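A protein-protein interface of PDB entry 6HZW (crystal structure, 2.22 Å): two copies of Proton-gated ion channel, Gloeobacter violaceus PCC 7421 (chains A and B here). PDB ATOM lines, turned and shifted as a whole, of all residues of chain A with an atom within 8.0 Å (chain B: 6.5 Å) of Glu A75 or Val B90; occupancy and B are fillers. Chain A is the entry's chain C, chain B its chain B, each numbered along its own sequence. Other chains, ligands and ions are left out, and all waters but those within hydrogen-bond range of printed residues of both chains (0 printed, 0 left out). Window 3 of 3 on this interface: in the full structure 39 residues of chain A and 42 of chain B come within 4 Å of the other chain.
The backbone carbonyl oxygen of Val B90 lies close to the side-chain carboxylate of Glu A75, 2.6 Å away.
OD2 of Asp B91 lies within salt-bridge range of NH2 of Arg A179.
The backbone carbonyl oxygen (O) of Phe A78 is in hydrogen-bond range of the guanidinium group (NH1) of Arg B105 (2.8 Å).
The backbone carbonyl oxygen of Asp B88 sits at hydrogen-bond distance from the backbone NH of Arg B105 (2.9 Å).
The backbone carbonyl oxygen (O) of Leu B103 lies within hydrogen-bond range of the backbone NH (N) of Val B90.
O of Asp B91 is in hydrogen-bond range of N of Leu B103.
OE2 of Glu A181 is in salt-bridge range of NH2 of Arg A77, at 3.8 Å.
OE1 of Glu A181 is in salt-bridge range of NE of Arg A133.
O of Ser A134 is in hydrogen-bond range of NH2 of Arg A179 (3.4 Å).
Among the printed residues, pairs that only touch across the chains: Arg A133 with Leu B103 and Arg A77 with Val B90.
Of chain B, only Val B90 (2.6 Å) comes within 4 Å of Glu A75.
Printed residues of chain A within 4 Å of Val B90: Glu A75 and Arg A77.
Printed residues of chain A within 4 Å of Leu B103: Arg A133.
Printed residues of chain A within 4 Å of Arg B105: Phe A78 (2.8 Å).
Val A132 touches none of the printed residues of chain B.
Leu A142 touches none of the printed residues of chain B.
The nearest residue of chain B that does not touch Glu A75 is Val B89 (4.2 Å).
Of the 19 printed residues of chain A, 5 touch a printed residue of chain B.
Printed residues of chain A that touch a printed residue of chain B: Glu A75, Arg A77, Phe A78, Arg A133 and Arg A179.
Along chain A the printed residues that touch a printed residue of chain B span positions 75 to 179.
Hydrophobic or aromatic side chains of chain B within 4 Å of the printed part of chain A: Val B90 and Leu B103.
No position is printed for both chains.
Of the 5 pairs that touch across the chains among the printed residues, none has its exchanged pair printed and touching as well.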
ATOM      1  N   VAL A  18      29.708 -13.837   0.500  1.00  0.00           N
ATOM      2  CA  VAL A  18      29.762 -14.457   1.816  1.00  0.00           C
ATOM      3  C   VAL A  18      30.930 -15.462   1.765  1.00  0.00           C
ATOM      4  O   VAL A  18      30.871 -16.448   1.050  1.00  0.00           O
ATOM      5  CB  VAL A  18      28.418 -15.090   2.257  1.00  0.00           C
ATOM      6  CG1 VAL A  18      28.562 -15.774   3.605  1.00  0.00           C
ATOM      7  CG2 VAL A  18      27.388 -13.976   2.385  1.00  0.00           C
ATOM      8  N   LEU A  45      31.513 -17.889   8.717  1.00  0.00           N
ATOM      9  CA  LEU A  45      30.954 -17.012   7.682  1.00  0.00           C
ATOM     10  C   LEU A  45      31.550 -15.590   7.838  1.00  0.00           C
ATOM     11  O   LEU A  45      31.783 -15.105   8.980  1.00  0.00           O
ATOM     12  CB  LEU A  45      29.432 -16.978   7.699  1.00  0.00           C
ATOM     13  CG  LEU A  45      28.699 -18.315   7.516  1.00  0.00           C
ATOM     14  CD1 LEU A  45      27.246 -18.079   7.831  1.00  0.00           C
ATOM     15  CD2 LEU A  45      28.847 -18.946   6.120  1.00  0.00           C
ATOM     16  N   TRP A  72      21.751  -8.574  10.711  1.00  0.00           N
ATOM     17  CA  TRP A  72      21.404  -9.395   9.566  1.00  0.00           C
ATOM     18  C   TRP A  72      22.484 -10.486   9.417  1.00  0.00           C
ATOM     19  O   TRP A  72      23.683 -10.212   9.440  1.00  0.00           O
ATOM     20  CB  TRP A  72      21.374  -8.589   8.310  1.00  0.00           C
ATOM     21  CG  TRP A  72      21.043  -9.406   7.108  1.00  0.00           C
ATOM     22  CD1 TRP A  72      19.822  -9.691   6.675  1.00  0.00           C
ATOM     23  CD2 TRP A  72      21.964 -10.007   6.185  1.00  0.00           C
ATOM     24  NE1 TRP A  72      19.886 -10.418   5.522  1.00  0.00           N
ATOM     25  CE2 TRP A  72      21.191 -10.639   5.192  1.00  0.00           C
ATOM     26  CE3 TRP A  72      23.359 -10.049   6.094  1.00  0.00           C
ATOM     27  CZ2 TRP A  72      21.747 -11.316   4.103  1.00  0.00           C
ATOM     28  CZ3 TRP A  72      23.928 -10.719   4.993  1.00  0.00           C
ATOM     29  CH2 TRP A  72      23.111 -11.361   4.022  1.00  0.00           C
ATOM     30  N   ILE A  73      22.012 -11.722   9.209  1.00  0.00           N
ATOM     31  CA  ILE A  73      22.855 -12.898   8.962  1.00  0.00           C
ATOM     32  C   ILE A  73      22.334 -13.615   7.720  1.00  0.00           C
ATOM     33  O   ILE A  73      21.131 -13.833   7.591  1.00  0.00           O
ATOM     34  CB  ILE A  73      22.873 -13.732  10.219  1.00  0.00           C
ATOM     35  CG1 ILE A  73      23.361 -12.802  11.339  1.00  0.00           C
ATOM     36  CG2 ILE A  73      23.718 -15.003  10.028  1.00  0.00           C
ATOM     37  CD1 ILE A  73      23.876 -13.454  12.564  1.00  0.00           C
ATOM     38  N   PRO A  74      23.190 -13.988   6.760  1.00  0.00           N
ATOM     39  CA  PRO A  74      22.702 -14.776   5.604  1.00  0.00           C
ATOM     40  C   PRO A  74      22.172 -16.170   6.040  1.00  0.00           C
ATOM     41  O   PRO A  74      22.710 -16.817   6.923  1.00  0.00           O
ATOM     42  CB  PRO A  74      23.912 -14.893   4.715  1.00  0.00           C
ATOM     43  CG  PRO A  74      25.071 -14.714   5.618  1.00  0.00           C
ATOM     44  CD  PRO A  74      24.644 -13.829   6.759  1.00  0.00           C
ATOM     45  N   GLU A  75      21.083 -16.601   5.409  1.00  0.00           N
ATOM     46  CA  GLU A  75      20.507 -17.918   5.593  1.00  0.00           C
ATOM     47  C   GLU A  75      21.322 -18.892   4.752  1.00  0.00           C
ATOM     48  O   GLU A  75      21.045 -19.149   3.575  1.00  0.00           O
ATOM     49  CB  GLU A  75      19.035 -17.968   5.161  1.00  0.00           C
ATOM     50  CG  GLU A  75      18.059 -17.240   6.091  1.00  0.00           C
ATOM     51  CD  GLU A  75      16.639 -17.171   5.524  1.00  0.00           C
ATOM     52  OE1 GLU A  75      16.335 -17.722   4.416  1.00  0.00           O
ATOM     53  OE2 GLU A  75      15.812 -16.573   6.228  1.00  0.00           O
ATOM     54  N   ILE A  76      22.332 -19.472   5.419  1.00  0.00           N
ATOM     55  CA  ILE A  76      23.160 -20.531   4.819  1.00  0.00           C
ATOM     56  C   ILE A  76      22.554 -21.911   5.158  1.00  0.00           C
ATOM     57  O   ILE A  76      22.175 -22.176   6.285  1.00  0.00           O
ATOM     58  CB  ILE A  76      24.603 -20.450   5.295  1.00  0.00           C
ATOM     59  CG1 ILE A  76      25.169 -19.045   4.989  1.00  0.00           C
ATOM     60  CG2 ILE A  76      25.438 -21.558   4.673  1.00  0.00           C
ATOM     61  CD1 ILE A  76      25.228 -18.655   3.561  1.00  0.00           C
ATOM     62  N   ARG A  77      22.394 -22.747   4.146  1.00  0.00           N
ATOM     63  CA  ARG A  77      21.930 -24.125   4.350  1.00  0.00           C
ATOM     64  C   ARG A  77      22.853 -25.143   3.672  1.00  0.00           C
ATOM     65  O   ARG A  77      23.659 -24.805   2.822  1.00  0.00           O
ATOM     66  CB  ARG A  77      20.515 -24.327   3.849  1.00  0.00           C
ATOM     67  CG  ARG A  77      19.449 -23.511   4.622  1.00  0.00           C
ATOM     68  CD  ARG A  77      18.021 -23.675   4.072  1.00  0.00           C
ATOM     69  NE  ARG A  77      17.989 -23.206   2.675  1.00  0.00           N
ATOM     70  CZ  ARG A  77      17.985 -21.914   2.296  1.00  0.00           C
ATOM     71  NH1 ARG A  77      17.962 -20.950   3.210  1.00  0.00           N
ATOM     72  NH2 ARG A  77      18.044 -21.597   0.999  1.00  0.00           N
ATOM     73  N   PHE A  78      22.668 -26.407   4.070  1.00  0.00           N
ATOM     74  CA  PHE A  78      23.326 -27.540   3.439  1.00  0.00           C
ATOM     75  C   PHE A  78      22.310 -28.153   2.462  1.00  0.00           C
ATOM     76  O   PHE A  78      21.130 -28.288   2.778  1.00  0.00           O
ATOM     77  CB  PHE A  78      23.794 -28.575   4.457  1.00  0.00           C
ATOM     78  CG  PHE A  78      24.949 -28.105   5.271  1.00  0.00           C
ATOM     79  CD1 PHE A  78      26.202 -28.111   4.734  1.00  0.00           C
ATOM     80  CD2 PHE A  78      24.795 -27.586   6.525  1.00  0.00           C
ATOM     81  CE1 PHE A  78      27.273 -27.636   5.447  1.00  0.00           C
ATOM     82  CE2 PHE A  78      25.851 -27.087   7.223  1.00  0.00           C
ATOM     83  CZ  PHE A  78      27.092 -27.142   6.696  1.00  0.00           C
ATOM     84  N   ARG A  85      20.609 -28.782  10.007  1.00  0.00           N
ATOM     85  CA  ARG A  85      21.655 -28.934  10.992  1.00  0.00           C
ATOM     86  C   ARG A  85      21.249 -28.468  12.420  1.00  0.00           C
ATOM     87  O   ARG A  85      20.462 -27.587  12.573  1.00  0.00           O
ATOM     88  CB  ARG A  85      22.935 -28.229  10.537  1.00  0.00           C
ATOM     89  CG  ARG A  85      22.896 -26.704  10.670  1.00  0.00           C
ATOM     90  CD  ARG A  85      24.050 -26.112   9.865  1.00  0.00           C
ATOM     91  NE  ARG A  85      24.157 -24.634   9.988  1.00  0.00           N
ATOM     92  CZ  ARG A  85      23.591 -23.749   9.174  1.00  0.00           C
ATOM     93  NH1 ARG A  85      22.934 -24.160   8.133  1.00  0.00           N
ATOM     94  NH2 ARG A  85      23.791 -22.451   9.345  1.00  0.00           N
ATOM     95  N   ILE A 131      25.020 -23.885   0.608  1.00  0.00           N
ATOM     96  CA  ILE A 131      24.160 -23.107  -0.283  1.00  0.00           C
ATOM     97  C   ILE A 131      23.494 -21.873   0.334  1.00  0.00           C
ATOM     98  O   ILE A 131      23.223 -21.818   1.551  1.00  0.00           O
ATOM     99  CB  ILE A 131      23.136 -23.991  -1.014  1.00  0.00           C
ATOM    100  CG1 ILE A 131      22.736 -23.430  -2.354  1.00  0.00           C
ATOM    101  CG2 ILE A 131      21.904 -24.252  -0.174  1.00  0.00           C
ATOM    102  CD1 ILE A 131      22.005 -24.420  -3.218  1.00  0.00           C
ATOM    103  N   VAL A 132      23.295 -20.853  -0.519  1.00  0.00           N
ATOM    104  CA  VAL A 132      22.579 -19.631  -0.158  1.00  0.00           C
ATOM    105  C   VAL A 132      21.649 -19.203  -1.297  1.00  0.00           C
ATOM    106  O   VAL A 132      21.991 -19.341  -2.474  1.00  0.00           O
ATOM    107  CB  VAL A 132      23.477 -18.478   0.297  1.00  0.00           C
ATOM    108  CG1 VAL A 132      24.267 -17.881  -0.884  1.00  0.00           C
ATOM    109  CG2 VAL A 132      22.654 -17.412   1.011  1.00  0.00           C
ATOM    110  N   ARG A 133      20.469 -18.756  -0.929  1.00  0.00           N
ATOM    111  CA  ARG A 133      19.462 -18.281  -1.882  1.00  0.00           C
ATOM    112  C   ARG A 133      19.505 -16.731  -1.848  1.00  0.00           C
ATOM    113  O   ARG A 133      19.552 -16.113  -0.762  1.00  0.00           O
ATOM    114  CB  ARG A 133      18.069 -18.780  -1.534  1.00  0.00           C
ATOM    115  CG  ARG A 133      17.030 -18.418  -2.592  1.00  0.00           C
ATOM    116  CD  ARG A 133      15.674 -18.989  -2.349  1.00  0.00           C
ATOM    117  NE  ARG A 133      15.464 -19.578  -3.663  1.00  0.00           N
ATOM    118  CZ  ARG A 133      14.480 -19.362  -4.486  1.00  0.00           C
ATOM    119  NH1 ARG A 133      14.547 -19.985  -5.641  1.00  0.00           N
ATOM    120  NH2 ARG A 133      13.470 -18.616  -4.162  1.00  0.00           N
ATOM    121  N   SER A 134      19.476 -16.147  -3.037  1.00  0.00           N
ATOM    122  CA  SER A 134      19.480 -14.679  -3.177  1.00  0.00           C
ATOM    123  C   SER A 134      18.092 -14.127  -2.721  1.00  0.00           C
ATOM    124  O   SER A 134      17.047 -14.803  -2.730  1.00  0.00           O
ATOM    125  CB  SER A 134      19.728 -14.257  -4.621  1.00  0.00           C
ATOM    126  OG  SER A 134      21.121 -14.403  -4.950  1.00  0.00           O
ATOM    127  N   VAL A 135      18.123 -12.881  -2.313  1.00  0.00           N
ATOM    128  CA  VAL A 135      16.932 -12.140  -1.883  1.00  0.00           C
ATOM    129  C   VAL A 135      16.533 -11.078  -2.928  1.00  0.00           C
ATOM    130  O   VAL A 135      17.319 -10.820  -3.871  1.00  0.00           O
ATOM    131  CB  VAL A 135      17.088 -11.624  -0.439  1.00  0.00           C
ATOM    132  CG1 VAL A 135      17.369 -12.811   0.491  1.00  0.00           C
ATOM    133  CG2 VAL A 135      18.220 -10.623  -0.323  1.00  0.00           C
ATOM    134  N   ILE A 140      23.212 -12.952  -3.605  1.00  0.00           N
ATOM    135  CA  ILE A 140      24.218 -13.377  -2.618  1.00  0.00           C
ATOM    136  C   ILE A 140      25.000 -14.531  -3.219  1.00  0.00           C
ATOM    137  O   ILE A 140      24.460 -15.491  -3.820  1.00  0.00           O
ATOM    138  CB  ILE A 140      23.612 -13.766  -1.293  1.00  0.00           C
ATOM    139  CG1 ILE A 140      22.693 -12.667  -0.787  1.00  0.00           C
ATOM    140  CG2 ILE A 140      24.706 -14.061  -0.287  1.00  0.00           C
ATOM    141  CD1 ILE A 140      21.836 -13.128   0.372  1.00  0.00           C
ATOM    142  N   LEU A 142      28.614 -17.178  -2.794  1.00  0.00           N
ATOM    143  CA  LEU A 142      29.503 -17.794  -1.781  1.00  0.00           C
ATOM    144  C   LEU A 142      30.951 -17.876  -2.290  1.00  0.00           C
ATOM    145  O   LEU A 142      31.208 -18.037  -3.468  1.00  0.00           O
ATOM    146  CB  LEU A 142      29.048 -19.202  -1.324  1.00  0.00           C
ATOM    147  CG  LEU A 142      27.674 -19.314  -0.660  1.00  0.00           C
ATOM    148  CD1 LEU A 142      27.373 -20.784  -0.369  1.00  0.00           C
ATOM    149  CD2 LEU A 142      27.587 -18.501   0.596  1.00  0.00           C
ATOM    150  N   ARG A 179      14.991 -17.279  -8.506  1.00  0.00           N
ATOM    151  CA  ARG A 179      16.058 -16.655  -7.730  1.00  0.00           C
ATOM    152  C   ARG A 179      17.388 -17.322  -7.978  1.00  0.00           C
ATOM    153  O   ARG A 179      17.482 -18.488  -8.346  1.00  0.00           O
ATOM    154  CB  ARG A 179      15.832 -16.570  -6.245  1.00  0.00           C
ATOM    155  CG  ARG A 179      14.621 -15.775  -5.834  1.00  0.00           C
ATOM    156  CD  ARG A 179      14.924 -14.335  -5.582  1.00  0.00           C
ATOM    157  NE  ARG A 179      13.688 -13.651  -5.258  1.00  0.00           N
ATOM    158  CZ  ARG A 179      13.109 -13.644  -4.059  1.00  0.00           C
ATOM    159  NH1 ARG A 179      11.965 -12.981  -3.872  1.00  0.00           N
ATOM    160  NH2 ARG A 179      13.653 -14.268  -3.019  1.00  0.00           N
ATOM    161  N   GLU A 181      20.886 -18.953  -6.795  1.00  0.00           N
ATOM    162  CA  GLU A 181      21.325 -19.833  -5.761  1.00  0.00           C
ATOM    163  C   GLU A 181      22.862 -20.037  -5.951  1.00  0.00           C
ATOM    164  O   GLU A 181      23.347 -20.177  -7.096  1.00  0.00           O
ATOM    165  CB  GLU A 181      20.453 -21.106  -5.855  1.00  0.00           C
ATOM    166  CG  GLU A 181      20.219 -21.827  -4.547  1.00  0.00           C
ATOM    167  CD  GLU A 181      18.834 -21.739  -3.902  1.00  0.00           C
ATOM    168  OE1 GLU A 181      17.816 -21.392  -4.485  1.00  0.00           O
ATOM    169  OE2 GLU A 181      18.786 -22.118  -2.725  1.00  0.00           O
ATOM    170  N   PHE B  42      11.514 -28.150  -0.926  1.00  0.00           N
ATOM    171  CA  PHE B  42      10.952 -26.805  -0.806  1.00  0.00           C
ATOM    172  C   PHE B  42       9.444 -26.893  -0.936  1.00  0.00           C
ATOM    173  O   PHE B  42       8.948 -27.571  -1.858  1.00  0.00           O
ATOM    174  CB  PHE B  42      11.394 -25.842  -1.909  1.00  0.00           C
ATOM    175  CG  PHE B  42      12.732 -25.198  -1.707  1.00  0.00           C
ATOM    176  CD1 PHE B  42      13.143 -24.716  -0.480  1.00  0.00           C
ATOM    177  CD2 PHE B  42      13.573 -25.011  -2.788  1.00  0.00           C
ATOM    178  CE1 PHE B  42      14.384 -24.103  -0.346  1.00  0.00           C
ATOM    179  CE2 PHE B  42      14.780 -24.351  -2.662  1.00  0.00           C
ATOM    180  CZ  PHE B  42      15.190 -23.922  -1.447  1.00  0.00           C
ATOM    181  N   GLU B  67       8.276 -11.828   8.974  1.00  0.00           N
ATOM    182  CA  GLU B  67       8.373 -13.038   9.750  1.00  0.00           C
ATOM    183  C   GLU B  67       6.971 -13.660   9.881  1.00  0.00           C
ATOM    184  O   GLU B  67       5.954 -12.935   9.919  1.00  0.00           O
ATOM    185  CB  GLU B  67       8.928 -12.715  11.154  1.00  0.00           C
ATOM    186  CG  GLU B  67      10.313 -12.097  11.179  1.00  0.00           C
ATOM    187  CD  GLU B  67      11.434 -13.122  11.117  1.00  0.00           C
ATOM    188  OE1 GLU B  67      12.181 -13.137  10.124  1.00  0.00           O
ATOM    189  OE2 GLU B  67      11.573 -13.913  12.066  1.00  0.00           O
ATOM    190  N   ASP B  88      11.462 -25.117   8.119  1.00  0.00           N
ATOM    191  CA  ASP B  88      12.166 -23.853   8.353  1.00  0.00           C
ATOM    192  C   ASP B  88      11.819 -22.857   7.223  1.00  0.00           C
ATOM    193  O   ASP B  88      11.916 -23.165   6.049  1.00  0.00           O
ATOM    194  CB  ASP B  88      13.683 -24.062   8.469  1.00  0.00           C
ATOM    195  CG  ASP B  88      14.095 -24.704   9.814  1.00  0.00           C
ATOM    196  OD1 ASP B  88      13.821 -24.155  10.888  1.00  0.00           O
ATOM    197  OD2 ASP B  88      14.715 -25.764   9.779  1.00  0.00           O
ATOM    198  N   VAL B  89      11.284 -21.710   7.599  1.00  0.00           N
ATOM    199  CA  VAL B  89      10.893 -20.688   6.638  1.00  0.00           C
ATOM    200  C   VAL B  89      12.168 -20.091   6.018  1.00  0.00           C
ATOM    201  O   VAL B  89      13.070 -19.701   6.733  1.00  0.00           O
ATOM    202  CB  VAL B  89      10.058 -19.616   7.314  1.00  0.00           C
ATOM    203  CG1 VAL B  89       9.847 -18.442   6.366  1.00  0.00           C
ATOM    204  CG2 VAL B  89       8.711 -20.218   7.746  1.00  0.00           C
ATOM    205  N   VAL B  90      12.210 -20.030   4.690  1.00  0.00           N
ATOM    206  CA  VAL B  90      13.343 -19.468   3.961  1.00  0.00           C
ATOM    207  C   VAL B  90      13.054 -17.980   3.617  1.00  0.00           C
ATOM    208  O   VAL B  90      13.875 -17.160   3.853  1.00  0.00           O
ATOM    209  CB  VAL B  90      13.621 -20.238   2.672  1.00  0.00           C
ATOM    210  CG1 VAL B  90      14.679 -19.509   1.784  1.00  0.00           C
ATOM    211  CG2 VAL B  90      14.009 -21.665   3.001  1.00  0.00           C
ATOM    212  N   ASP B  91      11.851 -17.675   3.133  1.00  0.00           N
ATOM    213  CA  ASP B  91      11.455 -16.330   2.787  1.00  0.00           C
ATOM    214  C   ASP B  91       9.930 -16.125   2.794  1.00  0.00           C
ATOM    215  O   ASP B  91       9.177 -17.010   2.393  1.00  0.00           O
ATOM    216  CB  ASP B  91      12.018 -16.037   1.400  1.00  0.00           C
ATOM    217  CG  ASP B  91      12.008 -14.560   1.065  1.00  0.00           C
ATOM    218  OD1 ASP B  91      12.109 -13.753   2.018  1.00  0.00           O
ATOM    219  OD2 ASP B  91      11.931 -14.215  -0.133  1.00  0.00           O
ATOM    220  N   ILE B  92       9.507 -14.936   3.210  1.00  0.00           N
ATOM    221  CA  ILE B  92       8.166 -14.386   3.013  1.00  0.00           C
ATOM    222  C   ILE B  92       8.321 -12.997   2.401  1.00  0.00           C
ATOM    223  O   ILE B  92       8.880 -12.159   3.003  1.00  0.00           O
ATOM    224  CB  ILE B  92       7.367 -14.328   4.311  1.00  0.00           C
ATOM    225  CG1 ILE B  92       7.407 -15.686   4.980  1.00  0.00           C
ATOM    226  CG2 ILE B  92       5.946 -13.967   3.950  1.00  0.00           C
ATOM    227  CD1 ILE B  92       6.603 -15.842   6.250  1.00  0.00           C
ATOM    228  N   LEU B 103       8.082 -19.292   1.118  1.00  0.00           N
ATOM    229  CA  LEU B 103       8.980 -20.413   0.839  1.00  0.00           C
ATOM    230  C   LEU B 103       9.558 -21.013   2.101  1.00  0.00           C
ATOM    231  O   LEU B 103      10.201 -20.315   2.865  1.00  0.00           O
ATOM    232  CB  LEU B 103      10.115 -20.008  -0.101  1.00  0.00           C
ATOM    233  CG  LEU B 103      10.957 -21.192  -0.634  1.00  0.00           C
ATOM    234  CD1 LEU B 103      10.255 -22.185  -1.549  1.00  0.00           C
ATOM    235  CD2 LEU B 103      12.152 -20.601  -1.353  1.00  0.00           C
ATOM    236  N   GLU B 104       9.316 -22.315   2.281  1.00  0.00           N
ATOM    237  CA  GLU B 104       9.924 -23.095   3.361  1.00  0.00           C
ATOM    238  C   GLU B 104      10.669 -24.307   2.817  1.00  0.00           C
ATOM    239  O   GLU B 104      10.327 -24.842   1.765  1.00  0.00           O
ATOM    240  CB  GLU B 104       8.906 -23.562   4.421  1.00  0.00           C
ATOM    241  CG  GLU B 104       7.888 -24.596   3.897  1.00  0.00           C
ATOM    242  CD  GLU B 104       7.050 -25.271   4.987  1.00  0.00           C
ATOM    243  OE1 GLU B 104       6.251 -24.612   5.677  1.00  0.00           O
ATOM    244  OE2 GLU B 104       7.147 -26.507   5.118  1.00  0.00           O
ATOM    245  N   ARG B 105      11.671 -24.708   3.569  1.00  0.00           N
ATOM    246  CA  ARG B 105      12.356 -25.988   3.316  1.00  0.00           C
ATOM    247  C   ARG B 105      11.898 -26.940   4.410  1.00  0.00           C
ATOM    248  O   ARG B 105      11.874 -26.592   5.576  1.00  0.00           O
ATOM    249  CB  ARG B 105      13.858 -25.845   3.272  1.00  0.00           C
ATOM    250  CG  ARG B 105      14.530 -27.125   2.862  1.00  0.00           C
ATOM    251  CD  ARG B 105      15.962 -26.925   2.429  1.00  0.00           C
ATOM    252  NE  ARG B 105      16.603 -28.215   2.328  1.00  0.00           N
ATOM    253  CZ  ARG B 105      17.888 -28.418   2.093  1.00  0.00           C
ATOM    254  NH1 ARG B 105      18.709 -27.419   1.800  1.00  0.00           N
ATOM    255  NH2 ARG B 105      18.328 -29.658   2.059  1.00  0.00           N
